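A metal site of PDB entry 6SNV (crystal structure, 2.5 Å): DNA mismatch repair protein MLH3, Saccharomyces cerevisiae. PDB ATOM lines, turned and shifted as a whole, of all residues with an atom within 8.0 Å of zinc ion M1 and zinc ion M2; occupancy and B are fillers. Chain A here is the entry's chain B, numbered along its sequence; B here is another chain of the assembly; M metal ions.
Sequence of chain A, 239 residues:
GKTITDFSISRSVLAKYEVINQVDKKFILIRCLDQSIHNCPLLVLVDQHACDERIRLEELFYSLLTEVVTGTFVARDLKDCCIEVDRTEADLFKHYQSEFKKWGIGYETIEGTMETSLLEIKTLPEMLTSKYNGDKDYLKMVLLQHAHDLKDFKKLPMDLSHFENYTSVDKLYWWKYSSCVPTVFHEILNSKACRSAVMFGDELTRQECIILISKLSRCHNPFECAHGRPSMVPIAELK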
ATOM      1  N   ASP A  47      21.738  -5.099  27.648  1.00  0.00           N
ATOM      2  CA  ASP A  47      21.409  -4.213  26.528  1.00  0.00           C
ATOM      3  C   ASP A  47      22.499  -4.458  25.456  1.00  0.00           C
ATOM      4  O   ASP A  47      23.680  -4.225  25.717  1.00  0.00           O
ATOM      5  CB  ASP A  47      21.397  -2.751  27.011  1.00  0.00           C
ATOM      6  CG  ASP A  47      21.285  -1.661  25.954  1.00  0.00           C
ATOM      7  OD1 ASP A  47      21.172  -1.993  24.762  1.00  0.00           O
ATOM      8  OD2 ASP A  47      21.336  -0.469  26.328  1.00  0.00           O
ATOM      9  N   HIS A  49      23.167  -2.974  22.566  1.00  0.00           N
ATOM     10  CA  HIS A  49      23.822  -1.773  22.068  1.00  0.00           C
ATOM     11  C   HIS A  49      24.909  -1.318  23.042  1.00  0.00           C
ATOM     12  O   HIS A  49      26.048  -1.123  22.623  1.00  0.00           O
ATOM     13  CB  HIS A  49      22.814  -0.654  21.774  1.00  0.00           C
ATOM     14  CG  HIS A  49      23.469   0.638  21.395  1.00  0.00           C
ATOM     15  ND1 HIS A  49      24.025   0.827  20.149  1.00  0.00           N
ATOM     16  CD2 HIS A  49      23.692   1.733  22.151  1.00  0.00           C
ATOM     17  CE1 HIS A  49      24.527   2.054  20.168  1.00  0.00           C
ATOM     18  NE2 HIS A  49      24.363   2.630  21.356  1.00  0.00           N
ATOM     19  N   ALA A  50      24.546  -1.201  24.349  1.00  0.00           N
ATOM     20  CA  ALA A  50      25.464  -0.826  25.434  1.00  0.00           C
ATOM     21  C   ALA A  50      26.612  -1.816  25.540  1.00  0.00           C
ATOM     22  O   ALA A  50      27.747  -1.402  25.728  1.00  0.00           O
ATOM     23  CB  ALA A  50      24.714  -0.756  26.743  1.00  0.00           C
ATOM     24  N   GLU A  53      28.870  -1.306  22.313  1.00  0.00           N
ATOM     25  CA  GLU A  53      29.473   0.016  22.497  1.00  0.00           C
ATOM     26  C   GLU A  53      30.596  -0.021  23.547  1.00  0.00           C
ATOM     27  O   GLU A  53      31.659   0.575  23.317  1.00  0.00           O
ATOM     28  CB  GLU A  53      28.398   1.039  22.879  1.00  0.00           C
ATOM     29  CG  GLU A  53      28.897   2.416  23.277  1.00  0.00           C
ATOM     30  CD  GLU A  53      27.745   3.331  23.600  1.00  0.00           C
ATOM     31  OE1 GLU A  53      26.872   3.521  22.720  1.00  0.00           O
ATOM     32  OE2 GLU A  53      27.693   3.838  24.736  1.00  0.00           O
ATOM     33  N   ARG A  54      30.386  -0.739  24.671  1.00  0.00           N
ATOM     34  CA  ARG A  54      31.384  -0.880  25.730  1.00  0.00           C
ATOM     35  C   ARG A  54      32.638  -1.602  25.249  1.00  0.00           C
ATOM     36  O   ARG A  54      33.729  -1.163  25.583  1.00  0.00           O
ATOM     37  CB  ARG A  54      30.802  -1.596  26.949  1.00  0.00           C
ATOM     38  CG  ARG A  54      31.755  -1.589  28.127  1.00  0.00           C
ATOM     39  CD  ARG A  54      31.991  -0.165  28.505  1.00  0.00           C
ATOM     40  NE  ARG A  54      33.276   0.072  29.156  1.00  0.00           N
ATOM     41  CZ  ARG A  54      33.541   1.200  29.800  1.00  0.00           C
ATOM     42  NH1 ARG A  54      32.614   2.144  29.910  1.00  0.00           N
ATOM     43  NH2 ARG A  54      34.729   1.375  30.357  1.00  0.00           N
ATOM     44  N   ASN A 190      33.621   8.115  22.322  1.00  0.00           N
ATOM     45  CA  ASN A 190      32.302   7.710  22.795  1.00  0.00           C
ATOM     46  C   ASN A 190      31.354   7.643  21.591  1.00  0.00           C
ATOM     47  O   ASN A 190      30.607   6.667  21.456  1.00  0.00           O
ATOM     48  CB  ASN A 190      31.743   8.760  23.770  1.00  0.00           C
ATOM     49  CG  ASN A 190      32.224   8.710  25.196  1.00  0.00           C
ATOM     50  OD1 ASN A 190      33.112   7.935  25.585  1.00  0.00           O
ATOM     51  ND2 ASN A 190      31.630   9.564  26.021  1.00  0.00           N
ATOM     52  N   SER A 191      31.401   8.684  20.732  1.00  0.00           N
ATOM     53  CA  SER A 191      30.602   8.845  19.513  1.00  0.00           C
ATOM     54  C   SER A 191      30.938   7.763  18.483  1.00  0.00           C
ATOM     55  O   SER A 191      30.021   7.244  17.833  1.00  0.00           O
ATOM     56  CB  SER A 191      30.826  10.235  18.920  1.00  0.00           C
ATOM     57  OG  SER A 191      30.269  10.393  17.618  1.00  0.00           O
ATOM     58  N   ALA A 193      32.308   4.767  19.141  1.00  0.00           N
ATOM     59  CA  ALA A 193      31.842   3.525  19.749  1.00  0.00           C
ATOM     60  C   ALA A 193      30.342   3.368  19.543  1.00  0.00           C
ATOM     61  O   ALA A 193      29.905   2.341  19.017  1.00  0.00           O
ATOM     62  CB  ALA A 193      32.186   3.502  21.241  1.00  0.00           C
ATOM     63  N   CYS A 194      29.563   4.428  19.859  1.00  0.00           N
ATOM     64  CA  CYS A 194      28.102   4.454  19.733  1.00  0.00           C
ATOM     65  C   CYS A 194      27.610   4.194  18.309  1.00  0.00           C
ATOM     66  O   CYS A 194      26.690   3.409  18.113  1.00  0.00           O
ATOM     67  CB  CYS A 194      27.535   5.743  20.307  1.00  0.00           C
ATOM     68  SG  CYS A 194      25.725   5.783  20.402  1.00  0.00           S
ATOM     69  N   ARG A 195      28.229   4.859  17.319  1.00  0.00           N
ATOM     70  CA  ARG A 195      27.881   4.750  15.900  1.00  0.00           C
ATOM     71  C   ARG A 195      28.205   3.418  15.266  1.00  0.00           C
ATOM     72  O   ARG A 195      27.483   2.988  14.361  1.00  0.00           O
ATOM     73  CB  ARG A 195      28.538   5.869  15.094  1.00  0.00           C
ATOM     74  CG  ARG A 195      27.799   7.166  15.189  1.00  0.00           C
ATOM     75  CD  ARG A 195      26.589   7.260  14.267  1.00  0.00           C
ATOM     76  NE  ARG A 195      26.092   8.623  14.327  1.00  0.00           N
ATOM     77  CZ  ARG A 195      26.482   9.599  13.516  1.00  0.00           C
ATOM     78  NH1 ARG A 195      27.301   9.349  12.504  1.00  0.00           N
ATOM     79  NH2 ARG A 195      26.034  10.836  13.694  1.00  0.00           N
ATOM     80  N   SER A 196      29.314   2.788  15.691  1.00  0.00           N
ATOM     81  CA  SER A 196      29.787   1.514  15.182  1.00  0.00           C
ATOM     82  C   SER A 196      29.095   0.322  15.855  1.00  0.00           C
ATOM     83  O   SER A 196      29.152  -0.793  15.329  1.00  0.00           O
ATOM     84  CB  SER A 196      31.293   1.408  15.350  1.00  0.00           C
ATOM     85  OG  SER A 196      31.937   2.388  14.563  1.00  0.00           O
ATOM     86  N   ALA A 197      28.446   0.564  17.024  1.00  0.00           N
ATOM     87  CA  ALA A 197      27.755  -0.436  17.838  1.00  0.00           C
ATOM     88  C   ALA A 197      26.472  -0.923  17.199  1.00  0.00           C
ATOM     89  O   ALA A 197      25.858  -0.191  16.414  1.00  0.00           O
ATOM     90  CB  ALA A 197      27.462   0.107  19.231  1.00  0.00           C
ATOM     91  N   VAL A 198      26.086  -2.163  17.539  1.00  0.00           N
ATOM     92  CA  VAL A 198      24.864  -2.837  17.098  1.00  0.00           C
ATOM     93  C   VAL A 198      23.656  -2.094  17.687  1.00  0.00           C
ATOM     94  O   VAL A 198      23.770  -1.539  18.783  1.00  0.00           O
ATOM     95  CB  VAL A 198      24.923  -4.376  17.435  1.00  0.00           C
ATOM     96  CG1 VAL A 198      24.718  -4.678  18.925  1.00  0.00           C
ATOM     97  CG2 VAL A 198      23.974  -5.184  16.568  1.00  0.00           C
ATOM     98  N   MET A 199      22.527  -2.041  16.976  1.00  0.00           N
ATOM     99  CA  MET A 199      21.365  -1.299  17.467  1.00  0.00           C
ATOM    100  C   MET A 199      20.178  -2.157  17.905  1.00  0.00           C
ATOM    101  O   MET A 199      20.166  -3.369  17.666  1.00  0.00           O
ATOM    102  CB  MET A 199      20.907  -0.312  16.404  1.00  0.00           C
ATOM    103  CG  MET A 199      21.258   1.118  16.711  1.00  0.00           C
ATOM    104  SD  MET A 199      20.644   2.275  15.453  1.00  0.00           S
ATOM    105  CE  MET A 199      18.809   2.114  15.692  1.00  0.00           C
ATOM    106  N   GLU A 224      28.608  -0.674  32.355  1.00  0.00           N
ATOM    107  CA  GLU A 224      28.080   0.588  31.817  1.00  0.00           C
ATOM    108  C   GLU A 224      28.515   0.850  30.395  1.00  0.00           C
ATOM    109  O   GLU A 224      29.592   0.402  29.995  1.00  0.00           O
ATOM    110  CB  GLU A 224      28.373   1.794  32.733  1.00  0.00           C
ATOM    111  CG  GLU A 224      29.817   2.227  32.780  1.00  0.00           C
ATOM    112  CD  GLU A 224      30.052   3.529  33.498  1.00  0.00           C
ATOM    113  OE1 GLU A 224      29.557   3.680  34.647  1.00  0.00           O
ATOM    114  OE2 GLU A 224      30.733   4.411  32.918  1.00  0.00           O
ATOM    115  N   CYS A 225      27.697   1.587  29.622  1.00  0.00           N
ATOM    116  CA  CYS A 225      27.959   1.984  28.238  1.00  0.00           C
ATOM    117  C   CYS A 225      29.058   3.069  28.200  1.00  0.00           C
ATOM    118  O   CYS A 225      29.703   3.326  29.222  1.00  0.00           O
ATOM    119  CB  CYS A 225      26.671   2.457  27.568  1.00  0.00           C
ATOM    120  SG  CYS A 225      25.999   3.994  28.265  1.00  0.00           S
ATOM    121  N   ALA A 226      29.272   3.718  27.037  1.00  0.00           N
ATOM    122  CA  ALA A 226      30.268   4.789  26.918  1.00  0.00           C
ATOM    123  C   ALA A 226      29.845   6.038  27.700  1.00  0.00           C
ATOM    124  O   ALA A 226      30.664   6.631  28.420  1.00  0.00           O
ATOM    125  CB  ALA A 226      30.516   5.125  25.450  1.00  0.00           C
ATOM    126  N   HIS A 227      28.546   6.397  27.621  1.00  0.00           N
ATOM    127  CA  HIS A 227      27.927   7.567  28.236  1.00  0.00           C
ATOM    128  C   HIS A 227      27.524   7.368  29.725  1.00  0.00           C
ATOM    129  O   HIS A 227      26.689   8.120  30.231  1.00  0.00           O
ATOM    130  CB  HIS A 227      26.721   8.031  27.383  1.00  0.00           C
ATOM    131  CG  HIS A 227      27.061   8.275  25.943  1.00  0.00           C
ATOM    132  ND1 HIS A 227      27.198   7.229  25.041  1.00  0.00           N
ATOM    133  CD2 HIS A 227      27.313   9.436  25.299  1.00  0.00           C
ATOM    134  CE1 HIS A 227      27.518   7.789  23.880  1.00  0.00           C
ATOM    135  NE2 HIS A 227      27.599   9.111  23.980  1.00  0.00           N
ATOM    136  N   GLY A 228      28.162   6.420  30.395  1.00  0.00           N
ATOM    137  CA  GLY A 228      27.971   6.122  31.814  1.00  0.00           C
ATOM    138  C   GLY A 228      26.621   5.620  32.302  1.00  0.00           C
ATOM    139  O   GLY A 228      26.325   5.747  33.493  1.00  0.00           O
ATOM    140  N   ARG A 229      25.803   5.015  31.412  1.00  0.00           N
ATOM    141  CA  ARG A 229      24.490   4.436  31.766  1.00  0.00           C
ATOM    142  C   ARG A 229      24.617   2.906  31.874  1.00  0.00           C
ATOM    143  O   ARG A 229      25.506   2.362  31.201  1.00  0.00           O
ATOM    144  CB  ARG A 229      23.422   4.839  30.739  1.00  0.00           C
ATOM    145  CG  ARG A 229      23.235   6.333  30.693  1.00  0.00           C
ATOM    146  CD  ARG A 229      22.125   6.736  29.752  1.00  0.00           C
ATOM    147  NE  ARG A 229      22.002   8.185  29.635  1.00  0.00           N
ATOM    148  CZ  ARG A 229      21.222   8.932  30.405  1.00  0.00           C
ATOM    149  NH1 ARG A 229      20.487   8.373  31.358  1.00  0.00           N
ATOM    150  NH2 ARG A 229      21.166  10.245  30.218  1.00  0.00           N
ATOM    151  N   PRO A 230      23.820   2.187  32.707  1.00  0.00           N
ATOM    152  CA  PRO A 230      24.008   0.727  32.838  1.00  0.00           C
ATOM    153  C   PRO A 230      23.840  -0.061  31.547  1.00  0.00           C
ATOM    154  O   PRO A 230      23.012   0.296  30.707  1.00  0.00           O
ATOM    155  CB  PRO A 230      22.965   0.305  33.877  1.00  0.00           C
ATOM    156  CG  PRO A 230      21.941   1.389  33.838  1.00  0.00           C
ATOM    157  CD  PRO A 230      22.719   2.639  33.586  1.00  0.00           C
ATOM    158  N   ARG B 264      17.453   6.361  26.449  1.00  0.00           N
ATOM    159  CA  ARG B 264      18.457   7.324  25.991  1.00  0.00           C
ATOM    160  C   ARG B 264      19.818   6.720  26.323  1.00  0.00           C
ATOM    161  O   ARG B 264      20.099   6.423  27.482  1.00  0.00           O
ATOM    162  CB  ARG B 264      18.259   8.704  26.648  1.00  0.00           C
ATOM    163  CG  ARG B 264      16.992   9.416  26.177  1.00  0.00           C
ATOM    164  CD  ARG B 264      16.901  10.852  26.655  1.00  0.00           C
ATOM    165  NE  ARG B 264      15.704  11.516  26.131  1.00  0.00           N
ATOM    166  CZ  ARG B 264      15.477  12.817  26.216  1.00  0.00           C
ATOM    167  NH1 ARG B 264      14.362  13.327  25.711  1.00  0.00           N
ATOM    168  NH2 ARG B 264      16.351  13.629  26.805  1.00  0.00           N
ATOM    169  N   CYS B 265      20.621   6.467  25.285  1.00  0.00           N
ATOM    170  CA  CYS B 265      21.951   5.878  25.433  1.00  0.00           C
ATOM    171  C   CYS B 265      22.978   6.925  25.896  1.00  0.00           C
ATOM    172  O   CYS B 265      23.083   7.994  25.252  1.00  0.00           O
ATOM    173  CB  CYS B 265      22.387   5.194  24.137  1.00  0.00           C
ATOM    174  SG  CYS B 265      24.105   4.639  24.158  1.00  0.00           S
ATOM    175  OXT CYS B 265      23.683   6.654  26.887  1.00  0.00           O
HETATM  176 ZN    ZN M   1      25.261   4.400  22.334  1.00  0.00          ZN
HETATM  177 ZN    ZN M   2      25.844   5.063  25.709  1.00  0.00          ZN
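The chain-end carboxylate (OXT) of Cys 265 of chain B lies within salt-bridge range of the guanidinium group (NE) of Arg 229 (3.6 Å). O of Val 198 lies within hydrogen-bond range of ND1 of His 49, at 2.7 Å. The guanidinium group of Arg 54 sits at hydrogen-bond distance from the backbone carbonyl oxygen of Cys 225, 3.2 Å away. N of His 227 lies close to SG of Cys 225 (3.6 Å). OE2 of Glu 53 sits close to ND1 of His 227 (3.4 Å). The backbone NH of His 49 sits at hydrogen-bond distance from the side-chain carboxylate of Asp 47 (3.1 Å). OE2 of Glu 53 lies close to N of Ala 226. The side-chain sulfur of Cys 225 lies close to the backbone NH of Arg 229.
Of the 23 residues printed, 4 come within 4 Å of zinc ion M1. The nearest printed residue that does not touch zinc ion M1 is His 227 (4.4 Å).
Ala 226 touches zinc ion M2. Of the 23 residues printed, 5 come within 4 Å of zinc ion M2. Along chain A the residues within 4 Å of zinc ion M2 span positions 53 to 227.
Zinc ion M1 is bound by OE1 of Glu 53 (1.9 Å), SG of Cys 265 of chain B (2.2 Å), NE2 of His 49 (2.2 Å) and SG of Cys 194 (2.4 Å). Zinc ion M1 has four donor atoms within binding distance.
Zinc ion M2 is bound by SG of Cys 265 of chain B (2.4 Å), OE2 of Glu 53 (2.4 Å) and SG of Cys 225 (2.8 Å). Zinc ion M2 has three donor atoms within binding distance. Slightly farther from zinc ion M2 lies a ring nitrogen (ND1) of His 227 (2.6 Å).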
